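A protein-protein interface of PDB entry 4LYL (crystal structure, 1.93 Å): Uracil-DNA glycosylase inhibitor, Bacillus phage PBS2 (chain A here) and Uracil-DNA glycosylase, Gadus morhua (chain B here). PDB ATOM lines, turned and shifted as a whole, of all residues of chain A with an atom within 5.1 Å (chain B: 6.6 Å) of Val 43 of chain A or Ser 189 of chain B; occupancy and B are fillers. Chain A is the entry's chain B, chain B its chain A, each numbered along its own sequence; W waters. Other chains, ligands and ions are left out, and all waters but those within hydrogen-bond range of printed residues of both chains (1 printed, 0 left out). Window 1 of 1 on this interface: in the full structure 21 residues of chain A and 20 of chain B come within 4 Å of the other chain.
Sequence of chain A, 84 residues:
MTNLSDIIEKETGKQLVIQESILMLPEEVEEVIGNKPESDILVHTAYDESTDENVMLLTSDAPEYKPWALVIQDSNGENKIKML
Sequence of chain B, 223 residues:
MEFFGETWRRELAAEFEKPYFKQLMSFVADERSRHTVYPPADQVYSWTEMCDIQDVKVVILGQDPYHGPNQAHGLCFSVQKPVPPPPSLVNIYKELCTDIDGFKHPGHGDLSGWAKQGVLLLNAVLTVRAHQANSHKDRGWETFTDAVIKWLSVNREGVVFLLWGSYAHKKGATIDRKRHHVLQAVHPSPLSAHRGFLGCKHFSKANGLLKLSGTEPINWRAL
The backbone NH (N) of Leu 191 of chain B sits at hydrogen-bond distance from the side-chain sulfur (SD) of Met 56 of chain A (3.4 Å).
OG of Ser 88 of chain B is in hydrogen-bond range of OE2 of Glu 20 of chain A.
The backbone NH (N) of Val 43 of chain A sits at hydrogen-bond distance from the backbone carbonyl oxygen (O) of Ile 22 of chain A, 2.7 Å away.
O of Glu 20 of chain A lies within hydrogen-bond range of N of Thr 45 of chain A.
N of Met 24 of chain A lies within hydrogen-bond range of O of Ile 41 of chain A (2.6 Å).
The side-chain hydroxyl of Ser 88 of chain B sits close to the backbone NH of Ser 189 of chain B (3.3 Å).
N of Leu 191 of chain B sits close to OG of Ser 189 of chain B (3.4 Å).
A ring nitrogen (ND1) of His 187 of chain B is in hydrogen-bond range of the backbone NH of Ser 189 of chain B.
OE1 of Glu 20 of chain A touches CD of Pro 87 of chain B, 3.6 Å away.
CG2 of Ile 22 of chain A touches NE2 of His 187 of chain B, 3.2 Å away.
Ser 189 of chain B touches Met 24 of chain A.
Ser 192 of chain B touches Met 24 of chain A (OG to CE, 3.8 Å).
Val 29 of chain A touches Leu 191 of chain B (CG2 to CD2, 3.9 Å).
Ser 189 of chain B touches Val 43 of chain A.
CG2 of Val 43 of chain A touches CD2 of Leu 191 of chain B, 3.5 Å away.
Thr 45 of chain A touches Pro 87 of chain B.
Of the printed residues of chain B, Val 29 of chain A touches Leu 191 (3.9 Å).
Val 43 of chain A touches two residues of chain B.
Printed residues of chain B within 4 Å of Thr 45 of chain A: Pro 87 (3.5 Å).
Printed residues of chain A within 4 Å of Ser 88 of chain B: Glu 20 (2.7 Å).
Of chain A, only Met 24 (3.7 Å) and Val 43 (3.7 Å) come within 4 Å of Ser 189 of chain B.
The nearest residue of chain B that does not touch Val 43 of chain A is Pro 190 of chain B (6.2 Å).
The nearest residue of chain A that does not touch Ser 189 of chain B is Ile 22 of chain A (4.2 Å).
The nearest printed residue of chain A that does not touch Pro 87 of chain B is Met 56 of chain A (7.1 Å).
Along chain B the printed residues that touch a printed residue of chain A span positions 87 to 192.
Of the 14 printed residues of chain A, 7 touch a printed residue of chain B.
Hydrophobic or aromatic side chains of chain A that line the printed part of chain B: Ile 22, Met 24, Val 29, Val 43 and Met 56.
Among the printed residues, 10 pairs touch across the chains.
Among the printed residues, no Asp or Glu carboxylate lies within 4 Å of a Lys or Arg side-chain nitrogen of the other chain.
Water W1 lies within hydrogen-bond range of OG1 of Thr 45 of chain A, OG of Ser 189 of chain B, OE2 of Glu 20 of chain A and O of Val 43 of chain A.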
ATOM      1  N   GLU A  20       4.677   5.674   3.101  1.00  0.00           N
ATOM      2  CA  GLU A  20       4.785   6.138   1.725  1.00  0.00           C
ATOM      3  C   GLU A  20       3.486   6.814   1.309  1.00  0.00           C
ATOM      4  O   GLU A  20       2.400   6.455   1.804  1.00  0.00           O
ATOM      5  CB  GLU A  20       5.048   4.965   0.800  1.00  0.00           C
ATOM      6  CG  GLU A  20       3.870   4.015   0.623  1.00  0.00           C
ATOM      7  CD  GLU A  20       4.111   2.936  -0.411  1.00  0.00           C
ATOM      8  OE1 GLU A  20       5.275   2.514  -0.482  1.00  0.00           O
ATOM      9  OE2 GLU A  20       3.159   2.511  -1.141  1.00  0.00           O
ATOM     10  N   SER A  21       3.627   7.750   0.372  1.00  0.00           N
ATOM     11  CA  SER A  21       2.575   8.533  -0.198  1.00  0.00           C
ATOM     12  C   SER A  21       2.698   8.548  -1.724  1.00  0.00           C
ATOM     13  O   SER A  21       3.605   9.177  -2.267  1.00  0.00           O
ATOM     14  CB  SER A  21       2.678   9.965   0.300  1.00  0.00           C
ATOM     15  OG  SER A  21       2.631  10.009   1.717  1.00  0.00           O
ATOM     16  N   ILE A  22       1.787   7.870  -2.404  1.00  0.00           N
ATOM     17  CA  ILE A  22       1.857   7.673  -3.870  1.00  0.00           C
ATOM     18  C   ILE A  22       0.787   8.508  -4.530  1.00  0.00           C
ATOM     19  O   ILE A  22      -0.363   8.348  -4.188  1.00  0.00           O
ATOM     20  CB  ILE A  22       1.609   6.202  -4.285  1.00  0.00           C
ATOM     21  CG1 ILE A  22       2.509   5.237  -3.542  1.00  0.00           C
ATOM     22  CG2 ILE A  22       1.755   6.023  -5.803  1.00  0.00           C
ATOM     23  CD1 ILE A  22       4.005   5.522  -3.653  1.00  0.00           C
ATOM     24  N   LEU A  23       1.143   9.408  -5.450  1.00  0.00           N
ATOM     25  CA  LEU A  23       0.154  10.150  -6.236  1.00  0.00           C
ATOM     26  C   LEU A  23      -0.516   9.309  -7.346  1.00  0.00           C
ATOM     27  O   LEU A  23       0.120   8.562  -8.127  1.00  0.00           O
ATOM     28  CB  LEU A  23       0.762  11.441  -6.812  1.00  0.00           C
ATOM     29  CG  LEU A  23      -0.218  12.537  -7.263  1.00  0.00           C
ATOM     30  CD1 LEU A  23      -0.934  13.175  -6.069  1.00  0.00           C
ATOM     31  CD2 LEU A  23       0.518  13.606  -8.051  1.00  0.00           C
ATOM     32  N   MET A  24      -1.839   9.434  -7.398  1.00  0.00           N
ATOM     33  CA  MET A  24      -2.626   8.745  -8.416  1.00  0.00           C
ATOM     34  C   MET A  24      -3.653   9.657  -9.048  1.00  0.00           C
ATOM     35  O   MET A  24      -4.333  10.419  -8.351  1.00  0.00           O
ATOM     36  CB  MET A  24      -3.396   7.570  -7.777  1.00  0.00           C
ATOM     37  CG  MET A  24      -2.477   6.440  -7.373  1.00  0.00           C
ATOM     38  SD  MET A  24      -3.182   4.819  -7.016  1.00  0.00           S
ATOM     39  CE  MET A  24      -1.780   4.204  -6.097  1.00  0.00           C
ATOM     40  N   VAL A  29      -7.778   5.530  -9.342  1.00  0.00           N
ATOM     41  CA  VAL A  29      -8.392   5.205  -8.047  1.00  0.00           C
ATOM     42  C   VAL A  29      -9.907   4.857  -8.105  1.00  0.00           C
ATOM     43  O   VAL A  29     -10.475   4.205  -7.190  1.00  0.00           O
ATOM     44  CB  VAL A  29      -8.183   6.454  -7.167  1.00  0.00           C
ATOM     45  CG1 VAL A  29      -9.149   6.518  -6.010  1.00  0.00           C
ATOM     46  CG2 VAL A  29      -6.723   6.524  -6.737  1.00  0.00           C
ATOM     47  N   ILE A  41      -4.992  12.146  -6.209  1.00  0.00           N
ATOM     48  CA  ILE A  41      -4.982  11.685  -4.835  1.00  0.00           C
ATOM     49  C   ILE A  41      -3.607  11.184  -4.480  1.00  0.00           C
ATOM     50  O   ILE A  41      -2.986  10.467  -5.251  1.00  0.00           O
ATOM     51  CB  ILE A  41      -5.970  10.526  -4.625  1.00  0.00           C
ATOM     52  CG1 ILE A  41      -7.420  10.995  -4.803  1.00  0.00           C
ATOM     53  CG2 ILE A  41      -5.772   9.920  -3.241  1.00  0.00           C
ATOM     54  CD1 ILE A  41      -7.979  11.854  -3.683  1.00  0.00           C
ATOM     55  N   LEU A  42      -3.165  11.571  -3.299  1.00  0.00           N
ATOM     56  CA  LEU A  42      -2.108  10.891  -2.568  1.00  0.00           C
ATOM     57  C   LEU A  42      -2.616   9.697  -1.736  1.00  0.00           C
ATOM     58  O   LEU A  42      -3.454   9.844  -0.795  1.00  0.00           O
ATOM     59  CB  LEU A  42      -1.363  11.876  -1.685  1.00  0.00           C
ATOM     60  CG  LEU A  42      -0.472  12.869  -2.460  1.00  0.00           C
ATOM     61  CD1 LEU A  42       0.197  13.905  -1.566  1.00  0.00           C
ATOM     62  CD2 LEU A  42       0.577  12.115  -3.229  1.00  0.00           C
ATOM     63  N   VAL A  43      -2.066   8.521  -2.070  1.00  0.00           N
ATOM     64  CA  VAL A  43      -2.352   7.289  -1.331  1.00  0.00           C
ATOM     65  C   VAL A  43      -1.284   7.125  -0.271  1.00  0.00           C
ATOM     66  O   VAL A  43      -0.169   6.682  -0.573  1.00  0.00           O
ATOM     67  CB  VAL A  43      -2.406   6.051  -2.245  1.00  0.00           C
ATOM     68  CG1 VAL A  43      -2.718   4.776  -1.451  1.00  0.00           C
ATOM     69  CG2 VAL A  43      -3.487   6.253  -3.274  1.00  0.00           C
ATOM     70  N   HIS A  44      -1.641   7.473   0.966  1.00  0.00           N
ATOM     71  CA  HIS A  44      -0.723   7.460   2.095  1.00  0.00           C
ATOM     72  C   HIS A  44      -0.917   6.145   2.854  1.00  0.00           C
ATOM     73  O   HIS A  44      -2.053   5.854   3.282  1.00  0.00           O
ATOM     74  CB  HIS A  44      -1.004   8.566   3.091  1.00  0.00           C
ATOM     75  CG  HIS A  44      -1.014   9.954   2.539  1.00  0.00           C
ATOM     76  ND1 HIS A  44       0.077  10.796   2.600  1.00  0.00           N
ATOM     77  CD2 HIS A  44      -2.032  10.687   2.042  1.00  0.00           C
ATOM     78  CE1 HIS A  44      -0.257  11.968   2.098  1.00  0.00           C
ATOM     79  NE2 HIS A  44      -1.528  11.922   1.734  1.00  0.00           N
ATOM     80  N   THR A  45       0.148   5.339   2.958  1.00  0.00           N
ATOM     81  CA  THR A  45       0.016   3.956   3.445  1.00  0.00           C
ATOM     82  C   THR A  45       0.835   3.635   4.669  1.00  0.00           C
ATOM     83  O   THR A  45       2.048   3.877   4.671  1.00  0.00           O
ATOM     84  CB  THR A  45       0.392   2.902   2.399  1.00  0.00           C
ATOM     85  OG1 THR A  45      -0.308   3.173   1.164  1.00  0.00           O
ATOM     86  CG2 THR A  45      -0.029   1.553   2.918  1.00  0.00           C
ATOM     87  N   MET A  56      -4.672   2.652   4.273  1.00  0.00           N
ATOM     88  CA  MET A  56      -4.485   3.779   3.352  1.00  0.00           C
ATOM     89  C   MET A  56      -5.455   4.945   3.561  1.00  0.00           C
ATOM     90  O   MET A  56      -6.675   4.772   3.531  1.00  0.00           O
ATOM     91  CB  MET A  56      -4.655   3.257   1.931  1.00  0.00           C
ATOM     92  CG  MET A  56      -3.683   2.160   1.602  1.00  0.00           C
ATOM     93  SD  MET A  56      -4.062   1.242   0.113  1.00  0.00           S
ATOM     94  CE  MET A  56      -5.080  -0.069   0.746  1.00  0.00           C
ATOM     95  N   LEU A  57      -4.897   6.137   3.738  1.00  0.00           N
ATOM     96  CA  LEU A  57      -5.625   7.395   3.838  1.00  0.00           C
ATOM     97  C   LEU A  57      -5.397   8.110   2.526  1.00  0.00           C
ATOM     98  O   LEU A  57      -4.280   8.462   2.175  1.00  0.00           O
ATOM     99  CB  LEU A  57      -5.081   8.223   5.018  1.00  0.00           C
ATOM    100  CG  LEU A  57      -5.893   9.505   5.280  1.00  0.00           C
ATOM    101  CD1 LEU A  57      -7.118   9.190   6.130  1.00  0.00           C
ATOM    102  CD2 LEU A  57      -5.055  10.543   5.979  1.00  0.00           C
ATOM    103  N   LEU A  58      -6.437   8.228   1.732  1.00  0.00           N
ATOM    104  CA  LEU A  58      -6.347   8.928   0.486  1.00  0.00           C
ATOM    105  C   LEU A  58      -6.636  10.401   0.738  1.00  0.00           C
ATOM    106  O   LEU A  58      -7.681  10.753   1.278  1.00  0.00           O
ATOM    107  CB  LEU A  58      -7.342   8.370  -0.508  1.00  0.00           C
ATOM    108  CG  LEU A  58      -6.997   7.040  -1.148  1.00  0.00           C
ATOM    109  CD1 LEU A  58      -6.939   5.893  -0.146  1.00  0.00           C
ATOM    110  CD2 LEU A  58      -8.054   6.783  -2.198  1.00  0.00           C
ATOM    111  N   PHE B  77      11.924   3.730  -4.942  1.00  0.00           N
ATOM    112  CA  PHE B  77      11.481   2.530  -4.176  1.00  0.00           C
ATOM    113  C   PHE B  77      12.311   1.945  -3.064  1.00  0.00           C
ATOM    114  O   PHE B  77      11.749   1.334  -2.118  1.00  0.00           O
ATOM    115  CB  PHE B  77      11.029   1.435  -5.124  1.00  0.00           C
ATOM    116  CG  PHE B  77       9.856   1.861  -5.911  1.00  0.00           C
ATOM    117  CD1 PHE B  77       8.654   2.169  -5.247  1.00  0.00           C
ATOM    118  CD2 PHE B  77       9.929   1.962  -7.289  1.00  0.00           C
ATOM    119  CE1 PHE B  77       7.546   2.566  -6.001  1.00  0.00           C
ATOM    120  CE2 PHE B  77       8.828   2.361  -8.027  1.00  0.00           C
ATOM    121  CZ  PHE B  77       7.634   2.645  -7.382  1.00  0.00           C
ATOM    122  N   PRO B  87       5.281  -0.272   1.757  1.00  0.00           N
ATOM    123  CA  PRO B  87       4.186  -1.032   1.110  1.00  0.00           C
ATOM    124  C   PRO B  87       4.257  -1.313  -0.409  1.00  0.00           C
ATOM    125  O   PRO B  87       3.934  -2.418  -0.843  1.00  0.00           O
ATOM    126  CB  PRO B  87       2.973  -0.196   1.424  1.00  0.00           C
ATOM    127  CG  PRO B  87       3.310   0.410   2.776  1.00  0.00           C
ATOM    128  CD  PRO B  87       4.741   0.813   2.607  1.00  0.00           C
ATOM    129  N   SER B  88       4.699  -0.364  -1.205  1.00  0.00           N
ATOM    130  CA  SER B  88       4.936  -0.605  -2.625  1.00  0.00           C
ATOM    131  C   SER B  88       6.098  -1.575  -2.828  1.00  0.00           C
ATOM    132  O   SER B  88       5.994  -2.473  -3.682  1.00  0.00           O
ATOM    133  CB  SER B  88       5.195   0.719  -3.339  1.00  0.00           C
ATOM    134  OG  SER B  88       3.982   1.426  -3.495  1.00  0.00           O
ATOM    135  N   ASN B  91       5.244  -5.124  -2.300  1.00  0.00           N
ATOM    136  CA  ASN B  91       4.583  -5.677  -3.482  1.00  0.00           C
ATOM    137  C   ASN B  91       5.519  -5.899  -4.661  1.00  0.00           C
ATOM    138  O   ASN B  91       5.306  -6.850  -5.419  1.00  0.00           O
ATOM    139  CB  ASN B  91       3.372  -4.842  -3.877  1.00  0.00           C
ATOM    140  CG  ASN B  91       2.186  -5.130  -2.996  1.00  0.00           C
ATOM    141  OD1 ASN B  91       2.009  -6.238  -2.534  1.00  0.00           O
ATOM    142  ND2 ASN B  91       1.389  -4.147  -2.763  1.00  0.00           N
ATOM    143  N   VAL B 186      -0.040  -0.882 -13.635  1.00  0.00           N
ATOM    144  CA  VAL B 186      -0.582  -0.015 -12.546  1.00  0.00           C
ATOM    145  C   VAL B 186       0.389  -0.005 -11.388  1.00  0.00           C
ATOM    146  O   VAL B 186       1.311  -0.838 -11.368  1.00  0.00           O
ATOM    147  CB  VAL B 186      -1.951  -0.446 -11.986  1.00  0.00           C
ATOM    148  CG1 VAL B 186      -3.061  -0.547 -13.044  1.00  0.00           C
ATOM    149  CG2 VAL B 186      -1.859  -1.716 -11.192  1.00  0.00           C
ATOM    150  N   HIS B 187       0.236   0.917 -10.424  1.00  0.00           N
ATOM    151  CA  HIS B 187       1.248   1.055  -9.322  1.00  0.00           C
ATOM    152  C   HIS B 187       1.314  -0.177  -8.383  1.00  0.00           C
ATOM    153  O   HIS B 187       0.283  -0.761  -8.097  1.00  0.00           O
ATOM    154  CB  HIS B 187       0.931   2.287  -8.499  1.00  0.00           C
ATOM    155  CG  HIS B 187       2.120   2.902  -7.834  1.00  0.00           C
ATOM    156  ND1 HIS B 187       2.628   2.433  -6.645  1.00  0.00           N
ATOM    157  CD2 HIS B 187       2.894   3.954  -8.185  1.00  0.00           C
ATOM    158  CE1 HIS B 187       3.731   3.091  -6.352  1.00  0.00           C
ATOM    159  NE2 HIS B 187       3.871   4.071  -7.229  1.00  0.00           N
ATOM    160  N   PRO B 188       2.508  -0.524  -7.854  1.00  0.00           N
ATOM    161  CA  PRO B 188       2.575  -1.564  -6.878  1.00  0.00           C
ATOM    162  C   PRO B 188       1.927  -1.208  -5.513  1.00  0.00           C
ATOM    163  O   PRO B 188       1.801  -2.082  -4.732  1.00  0.00           O
ATOM    164  CB  PRO B 188       4.091  -1.764  -6.674  1.00  0.00           C
ATOM    165  CG  PRO B 188       4.764  -0.558  -7.245  1.00  0.00           C
ATOM    166  CD  PRO B 188       3.850  -0.044  -8.276  1.00  0.00           C
ATOM    167  N   SER B 189       1.530   0.033  -5.269  1.00  0.00           N
ATOM    168  CA  SER B 189       0.854   0.429  -4.030  1.00  0.00           C
ATOM    169  C   SER B 189      -0.178  -0.671  -3.749  1.00  0.00           C
ATOM    170  O   SER B 189      -0.773  -1.243  -4.663  1.00  0.00           O
ATOM    171  CB  SER B 189       0.211   1.812  -4.163  1.00  0.00           C
ATOM    172  OG  SER B 189      -0.763   2.147  -3.160  1.00  0.00           O
ATOM    173  N   PRO B 190      -0.369  -1.010  -2.488  1.00  0.00           N
ATOM    174  CA  PRO B 190      -1.508  -1.856  -2.138  1.00  0.00           C
ATOM    175  C   PRO B 190      -2.897  -1.450  -2.670  1.00  0.00           C
ATOM    176  O   PRO B 190      -3.704  -2.349  -2.946  1.00  0.00           O
ATOM    177  CB  PRO B 190      -1.492  -1.870  -0.611  1.00  0.00           C
ATOM    178  CG  PRO B 190      -0.136  -1.448  -0.214  1.00  0.00           C
ATOM    179  CD  PRO B 190       0.394  -0.557  -1.307  1.00  0.00           C
ATOM    180  N   LEU B 191      -3.186  -0.155  -2.842  1.00  0.00           N
ATOM    181  CA  LEU B 191      -4.438   0.237  -3.461  1.00  0.00           C
ATOM    182  C   LEU B 191      -4.621  -0.415  -4.850  1.00  0.00           C
ATOM    183  O   LEU B 191      -5.737  -0.818  -5.174  1.00  0.00           O
ATOM    184  CB  LEU B 191      -4.595   1.759  -3.547  1.00  0.00           C
ATOM    185  CG  LEU B 191      -5.994   2.309  -3.871  1.00  0.00           C
ATOM    186  CD1 LEU B 191      -6.972   2.029  -2.726  1.00  0.00           C
ATOM    187  CD2 LEU B 191      -5.874   3.804  -4.065  1.00  0.00           C
ATOM    188  N   SER B 192      -3.531  -0.593  -5.620  1.00  0.00           N
ATOM    189  CA  SER B 192      -3.674  -1.077  -6.998  1.00  0.00           C
ATOM    190  C   SER B 192      -3.010  -2.391  -7.370  1.00  0.00           C
ATOM    191  O   SER B 192      -3.387  -2.992  -8.370  1.00  0.00           O
ATOM    192  CB  SER B 192      -3.241  -0.003  -7.990  1.00  0.00           C
ATOM    193  OG  SER B 192      -2.097   0.660  -7.540  1.00  0.00           O
ATOM    194  N   ALA B 193      -2.079  -2.881  -6.559  1.00  0.00           N
ATOM    195  CA  ALA B 193      -1.240  -3.999  -6.998  1.00  0.00           C
ATOM    196  C   ALA B 193      -1.923  -5.299  -7.449  1.00  0.00           C
ATOM    197  O   ALA B 193      -1.466  -5.947  -8.386  1.00  0.00           O
ATOM    198  CB  ALA B 193      -0.170  -4.304  -5.963  1.00  0.00           C
ATOM    199  N   HIS B 194      -3.010  -5.696  -6.796  1.00  0.00           N
ATOM    200  CA  HIS B 194      -3.712  -6.913  -7.208  1.00  0.00           C
ATOM    201  C   HIS B 194      -4.607  -6.641  -8.415  1.00  0.00           C
ATOM    202  O   HIS B 194      -5.497  -7.416  -8.752  1.00  0.00           O
ATOM    203  CB  HIS B 194      -4.563  -7.472  -6.052  1.00  0.00           C
ATOM    204  CG  HIS B 194      -3.775  -7.926  -4.861  1.00  0.00           C
ATOM    205  ND1 HIS B 194      -3.500  -9.258  -4.611  1.00  0.00           N
ATOM    206  CD2 HIS B 194      -3.253  -7.233  -3.820  1.00  0.00           C
ATOM    207  CE1 HIS B 194      -2.834  -9.359  -3.472  1.00  0.00           C
ATOM    208  NE2 HIS B 194      -2.654  -8.141  -2.985  1.00  0.00           N
ATOM    209  N   PHE B 197      -0.450  -5.104 -11.083  1.00  0.00           N
ATOM    210  CA  PHE B 197       0.979  -5.082 -10.804  1.00  0.00           C
ATOM    211  C   PHE B 197       1.435  -6.520 -10.521  1.00  0.00           C
ATOM    212  O   PHE B 197       2.352  -7.010 -11.174  1.00  0.00           O
ATOM    213  CB  PHE B 197       1.412  -4.092  -9.703  1.00  0.00           C
ATOM    214  CG  PHE B 197       2.880  -4.165  -9.447  1.00  0.00           C
ATOM    215  CD1 PHE B 197       3.774  -3.520 -10.304  1.00  0.00           C
ATOM    216  CD2 PHE B 197       3.381  -4.980  -8.455  1.00  0.00           C
ATOM    217  CE1 PHE B 197       5.136  -3.652 -10.130  1.00  0.00           C
ATOM    218  CE2 PHE B 197       4.756  -5.089  -8.264  1.00  0.00           C
ATOM    219  CZ  PHE B 197       5.627  -4.424  -9.096  1.00  0.00           C
HETATM  220  O   HOH W   1       0.560   3.815  -1.260  1.00  0.00           O
